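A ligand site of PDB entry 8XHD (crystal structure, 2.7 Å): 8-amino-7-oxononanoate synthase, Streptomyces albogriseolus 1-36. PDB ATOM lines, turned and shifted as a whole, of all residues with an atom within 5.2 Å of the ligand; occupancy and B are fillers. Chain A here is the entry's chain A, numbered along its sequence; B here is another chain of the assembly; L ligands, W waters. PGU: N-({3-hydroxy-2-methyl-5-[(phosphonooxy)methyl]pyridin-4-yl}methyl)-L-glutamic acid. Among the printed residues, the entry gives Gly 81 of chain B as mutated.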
ATOM      1  N   TYR A  51       6.785 -16.281 -13.775  1.00  0.00           N
ATOM      2  CA  TYR A  51       5.753 -17.040 -13.076  1.00  0.00           C
ATOM      3  C   TYR A  51       5.313 -18.285 -13.847  1.00  0.00           C
ATOM      4  O   TYR A  51       4.306 -18.893 -13.493  1.00  0.00           O
ATOM      5  CB  TYR A  51       4.540 -16.154 -12.745  1.00  0.00           C
ATOM      6  CG  TYR A  51       3.953 -15.370 -13.903  1.00  0.00           C
ATOM      7  CD1 TYR A  51       3.587 -15.989 -15.090  1.00  0.00           C
ATOM      8  CD2 TYR A  51       3.728 -13.996 -13.793  1.00  0.00           C
ATOM      9  CE1 TYR A  51       3.036 -15.278 -16.130  1.00  0.00           C
ATOM     10  CE2 TYR A  51       3.182 -13.271 -14.834  1.00  0.00           C
ATOM     11  CZ  TYR A  51       2.841 -13.921 -16.006  1.00  0.00           C
ATOM     12  OH  TYR A  51       2.290 -13.210 -17.047  1.00  0.00           O
ATOM     13  N   ASN A 109     -11.141 -13.410 -19.170  1.00  0.00           N
ATOM     14  CA  ASN A 109      -9.963 -12.731 -19.688  1.00  0.00           C
ATOM     15  C   ASN A 109      -8.813 -12.772 -18.686  1.00  0.00           C
ATOM     16  O   ASN A 109      -7.641 -12.778 -19.081  1.00  0.00           O
ATOM     17  CB  ASN A 109     -10.277 -11.274 -20.044  1.00  0.00           C
ATOM     18  CG  ASN A 109     -11.530 -11.125 -20.880  1.00  0.00           C
ATOM     19  OD1 ASN A 109     -12.452 -10.382 -20.502  1.00  0.00           O
ATOM     20  ND2 ASN A 109     -11.587 -11.811 -22.020  1.00  0.00           N
ATOM     21  N   SER A 110      -9.125 -12.789 -17.391  1.00  0.00           N
ATOM     22  CA  SER A 110      -8.110 -12.658 -16.348  1.00  0.00           C
ATOM     23  C   SER A 110      -8.683 -13.147 -15.025  1.00  0.00           C
ATOM     24  O   SER A 110      -9.907 -13.264 -14.853  1.00  0.00           O
ATOM     25  CB  SER A 110      -7.650 -11.201 -16.207  1.00  0.00           C
ATOM     26  OG  SER A 110      -8.748 -10.346 -15.983  1.00  0.00           O
ATOM     27  N   CYS A 111      -7.788 -13.429 -14.073  1.00  0.00           N
ATOM     28  CA  CYS A 111      -8.226 -13.726 -12.711  1.00  0.00           C
ATOM     29  C   CYS A 111      -8.851 -12.502 -12.066  1.00  0.00           C
ATOM     30  O   CYS A 111      -9.729 -12.633 -11.201  1.00  0.00           O
ATOM     31  CB  CYS A 111      -7.046 -14.223 -11.861  1.00  0.00           C
ATOM     32  SG  CYS A 111      -7.472 -14.778 -10.198  1.00  0.00           S
ATOM     33  N   SER A 112      -8.430 -11.314 -12.483  1.00  0.00           N
ATOM     34  CA  SER A 112      -9.005 -10.077 -11.974  1.00  0.00           C
ATOM     35  C   SER A 112     -10.485  -9.987 -12.340  1.00  0.00           C
ATOM     36  O   SER A 112     -11.316  -9.671 -11.485  1.00  0.00           O
ATOM     37  CB  SER A 112      -8.239  -8.878 -12.535  1.00  0.00           C
ATOM     38  OG  SER A 112      -6.837  -9.113 -12.485  1.00  0.00           O
ATOM     39  N   HIS A 142      -4.754 -10.494  -2.538  1.00  0.00           N
ATOM     40  CA  HIS A 142      -4.321  -9.711  -3.695  1.00  0.00           C
ATOM     41  C   HIS A 142      -5.316  -8.606  -3.992  1.00  0.00           C
ATOM     42  O   HIS A 142      -6.528  -8.772  -3.817  1.00  0.00           O
ATOM     43  CB  HIS A 142      -4.130 -10.608  -4.922  1.00  0.00           C
ATOM     44  CG  HIS A 142      -3.493  -9.916  -6.084  1.00  0.00           C
ATOM     45  ND1 HIS A 142      -4.226  -9.301  -7.070  1.00  0.00           N
ATOM     46  CD2 HIS A 142      -2.198  -9.733  -6.412  1.00  0.00           C
ATOM     47  CE1 HIS A 142      -3.407  -8.776  -7.965  1.00  0.00           C
ATOM     48  NE2 HIS A 142      -2.163  -9.025  -7.579  1.00  0.00           N
ATOM     49  N   CYS A 144      -6.557  -7.351  -6.566  1.00  0.00           N
ATOM     50  CA  CYS A 144      -7.653  -7.590  -7.492  1.00  0.00           C
ATOM     51  C   CYS A 144      -8.918  -7.979  -6.752  1.00  0.00           C
ATOM     52  O   CYS A 144     -10.020  -7.830  -7.290  1.00  0.00           O
ATOM     53  CB  CYS A 144      -7.267  -8.673  -8.500  1.00  0.00           C
ATOM     54  SG  CYS A 144      -7.349 -10.356  -7.858  1.00  0.00           S
ATOM     55  N   ASP A 184      -5.846 -15.647  -0.389  1.00  0.00           N
ATOM     56  CA  ASP A 184      -5.024 -16.272  -1.415  1.00  0.00           C
ATOM     57  C   ASP A 184      -4.568 -17.636  -0.916  1.00  0.00           C
ATOM     58  O   ASP A 184      -4.239 -17.795   0.262  1.00  0.00           O
ATOM     59  CB  ASP A 184      -3.804 -15.414  -1.774  1.00  0.00           C
ATOM     60  CG  ASP A 184      -4.181 -14.017  -2.215  1.00  0.00           C
ATOM     61  OD1 ASP A 184      -5.364 -13.647  -2.085  1.00  0.00           O
ATOM     62  OD2 ASP A 184      -3.285 -13.295  -2.695  1.00  0.00           O
ATOM     63  N   SER A 188       2.179 -14.491  -2.461  1.00  0.00           N
ATOM     64  CA  SER A 188       3.390 -14.032  -3.120  1.00  0.00           C
ATOM     65  C   SER A 188       3.979 -12.830  -2.392  1.00  0.00           C
ATOM     66  O   SER A 188       3.324 -12.185  -1.569  1.00  0.00           O
ATOM     67  CB  SER A 188       3.082 -13.685  -4.574  1.00  0.00           C
ATOM     68  OG  SER A 188       1.831 -13.023  -4.683  1.00  0.00           O
ATOM     69  N   ASP A 213      -7.734 -17.633  -3.939  1.00  0.00           N
ATOM     70  CA  ASP A 213      -7.072 -17.204  -5.170  1.00  0.00           C
ATOM     71  C   ASP A 213      -5.961 -18.213  -5.437  1.00  0.00           C
ATOM     72  O   ASP A 213      -4.905 -18.175  -4.810  1.00  0.00           O
ATOM     73  CB  ASP A 213      -6.526 -15.784  -5.038  1.00  0.00           C
ATOM     74  CG  ASP A 213      -6.149 -15.169  -6.376  1.00  0.00           C
ATOM     75  OD1 ASP A 213      -5.637 -15.899  -7.252  1.00  0.00           O
ATOM     76  OD2 ASP A 213      -6.357 -13.956  -6.551  1.00  0.00           O
ATOM     77  N   ALA A 215      -4.010 -18.558  -7.940  1.00  0.00           N
ATOM     78  CA  ALA A 215      -3.210 -18.131  -9.085  1.00  0.00           C
ATOM     79  C   ALA A 215      -1.794 -18.683  -9.043  1.00  0.00           C
ATOM     80  O   ALA A 215      -1.241 -19.061 -10.077  1.00  0.00           O
ATOM     81  CB  ALA A 215      -3.172 -16.598  -9.153  1.00  0.00           C
ATOM     82  N   HIS A 216      -1.190 -18.741  -7.858  1.00  0.00           N
ATOM     83  CA  HIS A 216       0.145 -19.289  -7.694  1.00  0.00           C
ATOM     84  C   HIS A 216       0.123 -20.701  -7.104  1.00  0.00           C
ATOM     85  O   HIS A 216       1.087 -21.133  -6.471  1.00  0.00           O
ATOM     86  CB  HIS A 216       1.004 -18.358  -6.846  1.00  0.00           C
ATOM     87  CG  HIS A 216       1.044 -16.952  -7.353  1.00  0.00           C
ATOM     88  ND1 HIS A 216       1.900 -16.551  -8.350  1.00  0.00           N
ATOM     89  CD2 HIS A 216       0.333 -15.862  -7.004  1.00  0.00           C
ATOM     90  CE1 HIS A 216       1.718 -15.265  -8.595  1.00  0.00           C
ATOM     91  NE2 HIS A 216       0.772 -14.821  -7.787  1.00  0.00           N
ATOM     92  N   SER A 245      -5.397 -17.928 -12.250  1.00  0.00           N
ATOM     93  CA  SER A 245      -4.899 -17.473 -13.539  1.00  0.00           C
ATOM     94  C   SER A 245      -4.422 -18.662 -14.353  1.00  0.00           C
ATOM     95  O   SER A 245      -3.994 -19.688 -13.798  1.00  0.00           O
ATOM     96  CB  SER A 245      -3.765 -16.453 -13.360  1.00  0.00           C
ATOM     97  OG  SER A 245      -4.211 -15.305 -12.672  1.00  0.00           O
ATOM     98  N   ASN A 247      -2.278 -17.952 -17.122  1.00  0.00           N
ATOM     99  CA  ASN A 247      -1.043 -17.501 -17.748  1.00  0.00           C
ATOM    100  C   ASN A 247       0.189 -17.875 -16.926  1.00  0.00           C
ATOM    101  O   ASN A 247       1.302 -17.868 -17.479  1.00  0.00           O
ATOM    102  CB  ASN A 247      -1.084 -15.987 -17.965  1.00  0.00           C
ATOM    103  CG  ASN A 247      -1.321 -15.209 -16.688  1.00  0.00           C
ATOM    104  OD1 ASN A 247      -1.941 -15.711 -15.753  1.00  0.00           O
ATOM    105  ND2 ASN A 247      -0.825 -13.989 -16.635  1.00  0.00           N
ATOM    106  N   LYS A 248       0.021 -18.180 -15.646  1.00  0.00           N
ATOM    107  CA  LYS A 248       1.100 -18.614 -14.779  1.00  0.00           C
ATOM    108  C   LYS A 248       0.933 -20.088 -14.475  1.00  0.00           C
ATOM    109  O   LYS A 248      -0.155 -20.521 -14.076  1.00  0.00           O
ATOM    110  CB  LYS A 248       1.121 -17.819 -13.475  1.00  0.00           C
ATOM    111  CG  LYS A 248       0.302 -16.535 -13.487  1.00  0.00           C
ATOM    112  CD  LYS A 248       0.326 -15.867 -12.128  1.00  0.00           C
ATOM    113  CE  LYS A 248      -0.633 -14.701 -12.061  1.00  0.00           C
ATOM    114  NZ  LYS A 248      -0.325 -13.667 -13.089  1.00  0.00           N
ATOM    115  N   GLY A 254      -5.400 -16.018 -19.763  1.00  0.00           N
ATOM    116  CA  GLY A 254      -6.680 -15.796 -19.115  1.00  0.00           C
ATOM    117  C   GLY A 254      -6.754 -16.335 -17.706  1.00  0.00           C
ATOM    118  O   GLY A 254      -5.765 -16.745 -17.091  1.00  0.00           O
ATOM    119  N   GLY A 255      -7.986 -16.324 -17.176  1.00  0.00           N
ATOM    120  CA  GLY A 255      -8.260 -16.788 -15.832  1.00  0.00           C
ATOM    121  C   GLY A 255      -9.509 -17.642 -15.778  1.00  0.00           C
ATOM    122  O   GLY A 255     -10.103 -17.946 -16.819  1.00  0.00           O
ATOM    123  N   GLU A 359      12.643  -9.352  -9.737  1.00  0.00           N
ATOM    124  CA  GLU A 359      11.768  -8.183  -9.731  1.00  0.00           C
ATOM    125  C   GLU A 359      11.815  -7.472  -8.382  1.00  0.00           C
ATOM    126  O   GLU A 359      11.790  -8.130  -7.335  1.00  0.00           O
ATOM    127  CB  GLU A 359      10.333  -8.594 -10.075  1.00  0.00           C
ATOM    128  CG  GLU A 359       9.754  -9.684  -9.196  1.00  0.00           C
ATOM    129  CD  GLU A 359       8.394 -10.172  -9.690  1.00  0.00           C
ATOM    130  OE1 GLU A 359       7.703  -9.399 -10.395  1.00  0.00           O
ATOM    131  OE2 GLU A 359       8.029 -11.318  -9.379  1.00  0.00           O
ATOM    132  N   ARG A 374      11.581 -10.551  -5.344  1.00  0.00           N
ATOM    133  CA  ARG A 374      10.687 -11.704  -5.462  1.00  0.00           C
ATOM    134  C   ARG A 374      11.267 -12.650  -6.504  1.00  0.00           C
ATOM    135  O   ARG A 374      11.129 -12.422  -7.715  1.00  0.00           O
ATOM    136  CB  ARG A 374       9.272 -11.270  -5.843  1.00  0.00           C
ATOM    137  CG  ARG A 374       8.205 -12.299  -5.481  1.00  0.00           C
ATOM    138  CD  ARG A 374       6.941 -12.131  -6.309  1.00  0.00           C
ATOM    139  NE  ARG A 374       6.511 -10.740  -6.383  1.00  0.00           N
ATOM    140  CZ  ARG A 374       5.410 -10.329  -7.001  1.00  0.00           C
ATOM    141  NH1 ARG A 374       4.589 -11.185  -7.574  1.00  0.00           N
ATOM    142  NH2 ARG A 374       5.123  -9.031  -7.026  1.00  0.00           N
ATOM    143  N   ARG A 376      11.142 -16.395  -8.233  1.00  0.00           N
ATOM    144  CA  ARG A 376      10.135 -17.405  -8.509  1.00  0.00           C
ATOM    145  C   ARG A 376      10.820 -18.589  -9.159  1.00  0.00           C
ATOM    146  O   ARG A 376      11.439 -18.445 -10.214  1.00  0.00           O
ATOM    147  CB  ARG A 376       9.009 -16.851  -9.396  1.00  0.00           C
ATOM    148  CG  ARG A 376       8.564 -15.448  -8.999  1.00  0.00           C
ATOM    149  CD  ARG A 376       7.112 -15.218  -9.336  1.00  0.00           C
ATOM    150  NE  ARG A 376       6.877 -13.854  -9.791  1.00  0.00           N
ATOM    151  CZ  ARG A 376       5.689 -13.266  -9.820  1.00  0.00           C
ATOM    152  NH1 ARG A 376       4.607 -13.880  -9.353  1.00  0.00           N
ATOM    153  NH2 ARG A 376       5.576 -12.047 -10.326  1.00  0.00           N
ATOM    154  N   LEU B  80       5.927 -11.580 -16.665  1.00  0.00           N
ATOM    155  CA  LEU B  80       6.149 -10.576 -15.628  1.00  0.00           C
ATOM    156  C   LEU B  80       5.117  -9.466 -15.798  1.00  0.00           C
ATOM    157  O   LEU B  80       4.524  -9.315 -16.875  1.00  0.00           O
ATOM    158  CB  LEU B  80       7.566  -9.987 -15.695  1.00  0.00           C
ATOM    159  CG  LEU B  80       8.752 -10.881 -15.334  1.00  0.00           C
ATOM    160  CD1 LEU B  80      10.066 -10.249 -15.735  1.00  0.00           C
ATOM    161  CD2 LEU B  80       8.742 -11.180 -13.845  1.00  0.00           C
ATOM    162  N   GLY B  81       4.918  -8.700 -14.739  1.00  0.00           N
ATOM    163  CA  GLY B  81       4.098  -7.505 -14.869  1.00  0.00           C
ATOM    164  C   GLY B  81       4.732  -6.530 -15.840  1.00  0.00           C
ATOM    165  O   GLY B  81       5.958  -6.391 -15.902  1.00  0.00           O
ATOM    166  N   ARG B  82       3.886  -5.839 -16.609  1.00  0.00           N
ATOM    167  CA  ARG B  82       4.382  -4.914 -17.634  1.00  0.00           C
ATOM    168  C   ARG B  82       5.178  -3.767 -17.032  1.00  0.00           C
ATOM    169  O   ARG B  82       5.880  -3.061 -17.765  1.00  0.00           O
ATOM    170  CB  ARG B  82       3.232  -4.345 -18.463  1.00  0.00           C
ATOM    171  CG  ARG B  82       2.338  -3.358 -17.748  1.00  0.00           C
ATOM    172  CD  ARG B  82       1.310  -2.785 -18.705  1.00  0.00           C
ATOM    173  NE  ARG B  82       1.942  -1.973 -19.741  1.00  0.00           N
ATOM    174  CZ  ARG B  82       1.412  -1.746 -20.944  1.00  0.00           C
ATOM    175  NH1 ARG B  82       0.267  -2.306 -21.301  1.00  0.00           N
ATOM    176  NH2 ARG B  82       2.060  -0.954 -21.796  1.00  0.00           N
ATOM    177  N   ASN B 109      -6.315  -6.256 -21.332  1.00  0.00           N
ATOM    178  CA  ASN B 109      -6.982  -7.455 -21.837  1.00  0.00           C
ATOM    179  C   ASN B 109      -8.476  -7.249 -22.077  1.00  0.00           C
ATOM    180  O   ASN B 109      -9.133  -8.182 -22.550  1.00  0.00           O
ATOM    181  CB  ASN B 109      -6.758  -8.623 -20.867  1.00  0.00           C
ATOM    182  CG  ASN B 109      -7.186  -8.319 -19.454  1.00  0.00           C
ATOM    183  OD1 ASN B 109      -8.281  -7.808 -19.219  1.00  0.00           O
ATOM    184  ND2 ASN B 109      -6.328  -8.640 -18.494  1.00  0.00           N
ATOM    185  N   MET B 279      -1.398  -2.571 -13.845  1.00  0.00           N
ATOM    186  CA  MET B 279      -0.182  -2.999 -13.164  1.00  0.00           C
ATOM    187  C   MET B 279      -0.138  -4.514 -12.977  1.00  0.00           C
ATOM    188  O   MET B 279       0.896  -5.146 -13.235  1.00  0.00           O
ATOM    189  CB  MET B 279      -0.055  -2.314 -11.805  1.00  0.00           C
ATOM    190  CG  MET B 279       1.089  -2.852 -10.957  1.00  0.00           C
ATOM    191  SD  MET B 279       1.260  -2.078  -9.334  1.00  0.00           S
ATOM    192  CE  MET B 279       1.718  -0.418  -9.793  1.00  0.00           C
ATOM    193  N   TRP B 280      -1.238  -5.114 -12.513  1.00  0.00           N
ATOM    194  CA  TRP B 280      -1.226  -6.485 -12.032  1.00  0.00           C
ATOM    195  C   TRP B 280      -1.992  -7.463 -12.908  1.00  0.00           C
ATOM    196  O   TRP B 280      -1.977  -8.671 -12.614  1.00  0.00           O
ATOM    197  CB  TRP B 280      -1.786  -6.547 -10.612  1.00  0.00           C
ATOM    198  CG  TRP B 280      -3.261  -6.221 -10.492  1.00  0.00           C
ATOM    199  CD1 TRP B 280      -4.301  -6.771 -11.191  1.00  0.00           C
ATOM    200  CD2 TRP B 280      -3.853  -5.292  -9.581  1.00  0.00           C
ATOM    201  NE1 TRP B 280      -5.486  -6.223 -10.795  1.00  0.00           N
ATOM    202  CE2 TRP B 280      -5.246  -5.314  -9.803  1.00  0.00           C
ATOM    203  CE3 TRP B 280      -3.337  -4.439  -8.608  1.00  0.00           C
ATOM    204  CZ2 TRP B 280      -6.127  -4.511  -9.091  1.00  0.00           C
ATOM    205  CZ3 TRP B 280      -4.204  -3.641  -7.904  1.00  0.00           C
ATOM    206  CH2 TRP B 280      -5.595  -3.686  -8.145  1.00  0.00           C
ATOM    207  N   SER B 281      -2.713  -7.001 -13.918  1.00  0.00           N
ATOM    208  CA  SER B 281      -3.523  -7.874 -14.752  1.00  0.00           C
ATOM    209  C   SER B 281      -2.817  -8.123 -16.076  1.00  0.00           C
ATOM    210  O   SER B 281      -2.299  -7.185 -16.685  1.00  0.00           O
ATOM    211  CB  SER B 281      -4.923  -7.296 -14.985  1.00  0.00           C
ATOM    212  OG  SER B 281      -5.824  -8.312 -15.401  1.00  0.00           O
ATOM    213  N   GLN B 282      -2.809  -9.386 -16.505  1.00  0.00           N
ATOM    214  CA  GLN B 282      -1.970  -9.831 -17.606  1.00  0.00           C
ATOM    215  C   GLN B 282      -2.190  -8.999 -18.866  1.00  0.00           C
ATOM    216  O   GLN B 282      -3.314  -8.596 -19.194  1.00  0.00           O
ATOM    217  CB  GLN B 282      -2.228 -11.302 -17.906  1.00  0.00           C
ATOM    218  CG  GLN B 282      -3.694 -11.643 -18.165  1.00  0.00           C
ATOM    219  CD  GLN B 282      -3.922 -13.125 -18.371  1.00  0.00           C
ATOM    220  OE1 GLN B 282      -3.704 -13.650 -19.467  1.00  0.00           O
ATOM    221  NE2 GLN B 282      -4.353 -13.803 -17.319  1.00  0.00           N
ATOM    222  N   ARG B 283      -1.092  -8.733 -19.571  1.00  0.00           N
ATOM    223  CA  ARG B 283      -1.125  -8.069 -20.855  1.00  0.00           C
ATOM    224  C   ARG B 283      -1.764  -8.977 -21.900  1.00  0.00           C
ATOM    225  O   ARG B 283      -1.932 -10.182 -21.707  1.00  0.00           O
ATOM    226  CB  ARG B 283       0.287  -7.693 -21.297  1.00  0.00           C
ATOM    227  CG  ARG B 283       1.061  -6.898 -20.254  1.00  0.00           C
ATOM    228  CD  ARG B 283       2.514  -7.351 -20.180  1.00  0.00           C
ATOM    229  NE  ARG B 283       2.652  -8.794 -20.076  1.00  0.00           N
ATOM    230  CZ  ARG B 283       2.379  -9.503 -18.985  1.00  0.00           C
ATOM    231  NH1 ARG B 283       1.914  -8.931 -17.887  1.00  0.00           N
ATOM    232  NH2 ARG B 283       2.589 -10.820 -18.997  1.00  0.00           N
HETATM  233  N1  PGU L   1      -4.116 -13.014  -7.979  1.00  0.00           N
HETATM  234  C2  PGU L   1      -2.809 -13.053  -7.714  1.00  0.00           C
HETATM  235  C2A PGU L   1      -2.347 -13.676  -6.435  1.00  0.00           C
HETATM  236  C3  PGU L   1      -1.881 -12.520  -8.618  1.00  0.00           C
HETATM  237  O3  PGU L   1      -0.551 -12.567  -8.320  1.00  0.00           O
HETATM  238  C4  PGU L   1      -2.335 -11.931  -9.804  1.00  0.00           C
HETATM  239  C4A PGU L   1      -1.366 -11.352 -10.805  1.00  0.00           C
HETATM  240  C5  PGU L   1      -3.711 -11.914 -10.066  1.00  0.00           C
HETATM  241  C6  PGU L   1      -4.554 -12.468  -9.112  1.00  0.00           C
HETATM  242  C5A PGU L   1      -4.256 -11.308 -11.323  1.00  0.00           C
HETATM  243  O4P PGU L   1      -4.358 -12.301 -12.388  1.00  0.00           O
HETATM  244  P   PGU L   1      -4.577 -11.849 -13.917  1.00  0.00           P
HETATM  245  O1P PGU L   1      -5.093 -13.083 -14.646  1.00  0.00           O
HETATM  246  O2P PGU L   1      -5.598 -10.736 -13.855  1.00  0.00           O
HETATM  247  O3P PGU L   1      -3.224 -11.409 -14.428  1.00  0.00           O
HETATM  248  N   PGU L   1      -0.079 -10.938 -10.226  1.00  0.00           N
HETATM  249  CA  PGU L   1       1.074 -11.055 -11.143  1.00  0.00           C
HETATM  250  CB  PGU L   1       1.030  -9.978 -12.241  1.00  0.00           C
HETATM  251  CG  PGU L   1       0.425 -10.479 -13.548  1.00  0.00           C
HETATM  252  CD  PGU L   1       0.795  -9.690 -14.783  1.00  0.00           C
HETATM  253  OE1 PGU L   1       0.603  -8.453 -14.775  1.00  0.00           O
HETATM  254  OE2 PGU L   1       1.269 -10.302 -15.757  1.00  0.00           O
HETATM  255  C   PGU L   1       2.431 -10.985 -10.424  1.00  0.00           C
HETATM  256  O   PGU L   1       2.748  -9.900  -9.892  1.00  0.00           O
HETATM  257  OXT PGU L   1       3.118 -12.023 -10.434  1.00  0.00           O
HETATM  258  O   HOH W   1       1.129  -6.655 -16.591  1.00  0.00           O
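The side-chain hydroxyl (OG) of Ser 112 is in hydrogen-bond range of the side-chain hydroxyl (OG) of Ser 281 of chain B, 3.2 Å away.
The guanidinium group (NH2) of Arg 376 lies within salt-bridge range of the side-chain carboxylate (OE2) of Glu 359 (2.7 Å).
The guanidinium group of Arg 283 of chain B is in hydrogen-bond range of the side-chain hydroxyl of Tyr 51.
The side-chain carboxylate (OD1) of Asp 213 lies within hydrogen-bond range of the side-chain sulfur (SG) of Cys 111, 3.6 Å away.
The side-chain amide nitrogen (NE2) of Gln 282 of chain B sits close to the side-chain amide oxygen (OD1) of Asn 247 (3.5 Å).
The guanidinium group (NE) of Arg 374 is in salt-bridge range of the side-chain carboxylate (OE2) of Glu 359 (3.4 Å).
The side-chain hydroxyl (OH) of Tyr 51 lies within hydrogen-bond range of the side-chain amide nitrogen (ND2) of Asn 247 (3.2 Å).
ND1 of His 142 is in hydrogen-bond range of N of Cys 144, 3.1 Å away.
Water W1 lies within hydrogen-bond range of an oxygen (OE1) of the ligand (2.6 Å), the guanidinium group (NH1) of Arg 283 of chain B (2.7 Å), the backbone NH (N) of Arg 82 of chain B (2.9 Å) and the backbone carbonyl oxygen (O) of Ser 281 of chain B (3.5 Å).
The backbone NH (N) of Ser 112 is in hydrogen-bond range of an oxygen (O2P) of the ligand (3.2 Å).
OG of Ser 112 is in hydrogen-bond range of O2P of the ligand, 2.5 Å away.
The guanidinium group of Arg 376 lies within salt-bridge range of an oxygen (OXT) of the ligand, 2.5 Å away.
An oxygen (OE2) of the ligand is in salt-bridge range of the guanidinium group (NH1) of Arg 283 of chain B (2.6 Å).
A ring nitrogen (NE2) of His 216 lies within hydrogen-bond range of an oxygen (O3) of the ligand.
The backbone NH (N) of Cys 111 lies within hydrogen-bond range of an oxygen (O1P) of the ligand, 2.8 Å away.
The side-chain carboxylate (OD2) of Asp 213 lies within hydrogen-bond range of a nitrogen (N1) of the ligand (2.8 Å).
An oxygen (O3P) of the ligand lies within hydrogen-bond range of the backbone NH (N) of Gln 282 of chain B (2.9 Å).
An oxygen (O1P) of the ligand is in hydrogen-bond range of the side-chain amide nitrogen (NE2) of Gln 282 of chain B.
OG of Ser 281 of chain B is in hydrogen-bond range of O2P of the ligand (2.9 Å).
The side-chain hydroxyl (OG) of Ser 245 is in hydrogen-bond range of an oxygen (O4P) of the ligand, 3.0 Å away.
The guanidinium group (NH1) of Arg 374 lies within salt-bridge range of an oxygen (O) of the ligand, 3.2 Å away.
An oxygen (O3P) of the ligand lies within salt-bridge range of the side-chain amino group (NZ) of Lys 248, 3.9 Å away.
OH of Tyr 51 sits at hydrogen-bond distance from OE2 of the ligand (3.3 Å).
An oxygen (OE1) of the ligand sits close to the backbone carbonyl oxygen (O) of Trp 280 of chain B (3.4 Å).
CB of Ser 110 touches O2P of the ligand (3.2 Å).
His 142 touches the ligand.
Cys 144 touches the ligand.
Asp 184 touches the ligand (OD2 to C2A, 3.9 Å).
Ala 215 touches the ligand (CB to C2, 3.8 Å).
O of Leu 80 of chain B touches OE2 of the ligand (3.6 Å).
CA of Gly 81 of chain B touches OE1 of the ligand, at 3.6 Å.
O of Met 279 of chain B touches OE1 of the ligand, 3.7 Å away.
Of the 29 residues printed, 21 come within 4 Å of the ligand.
The nearest printed residue that does not touch the ligand is Asn 247 (4.2 Å).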
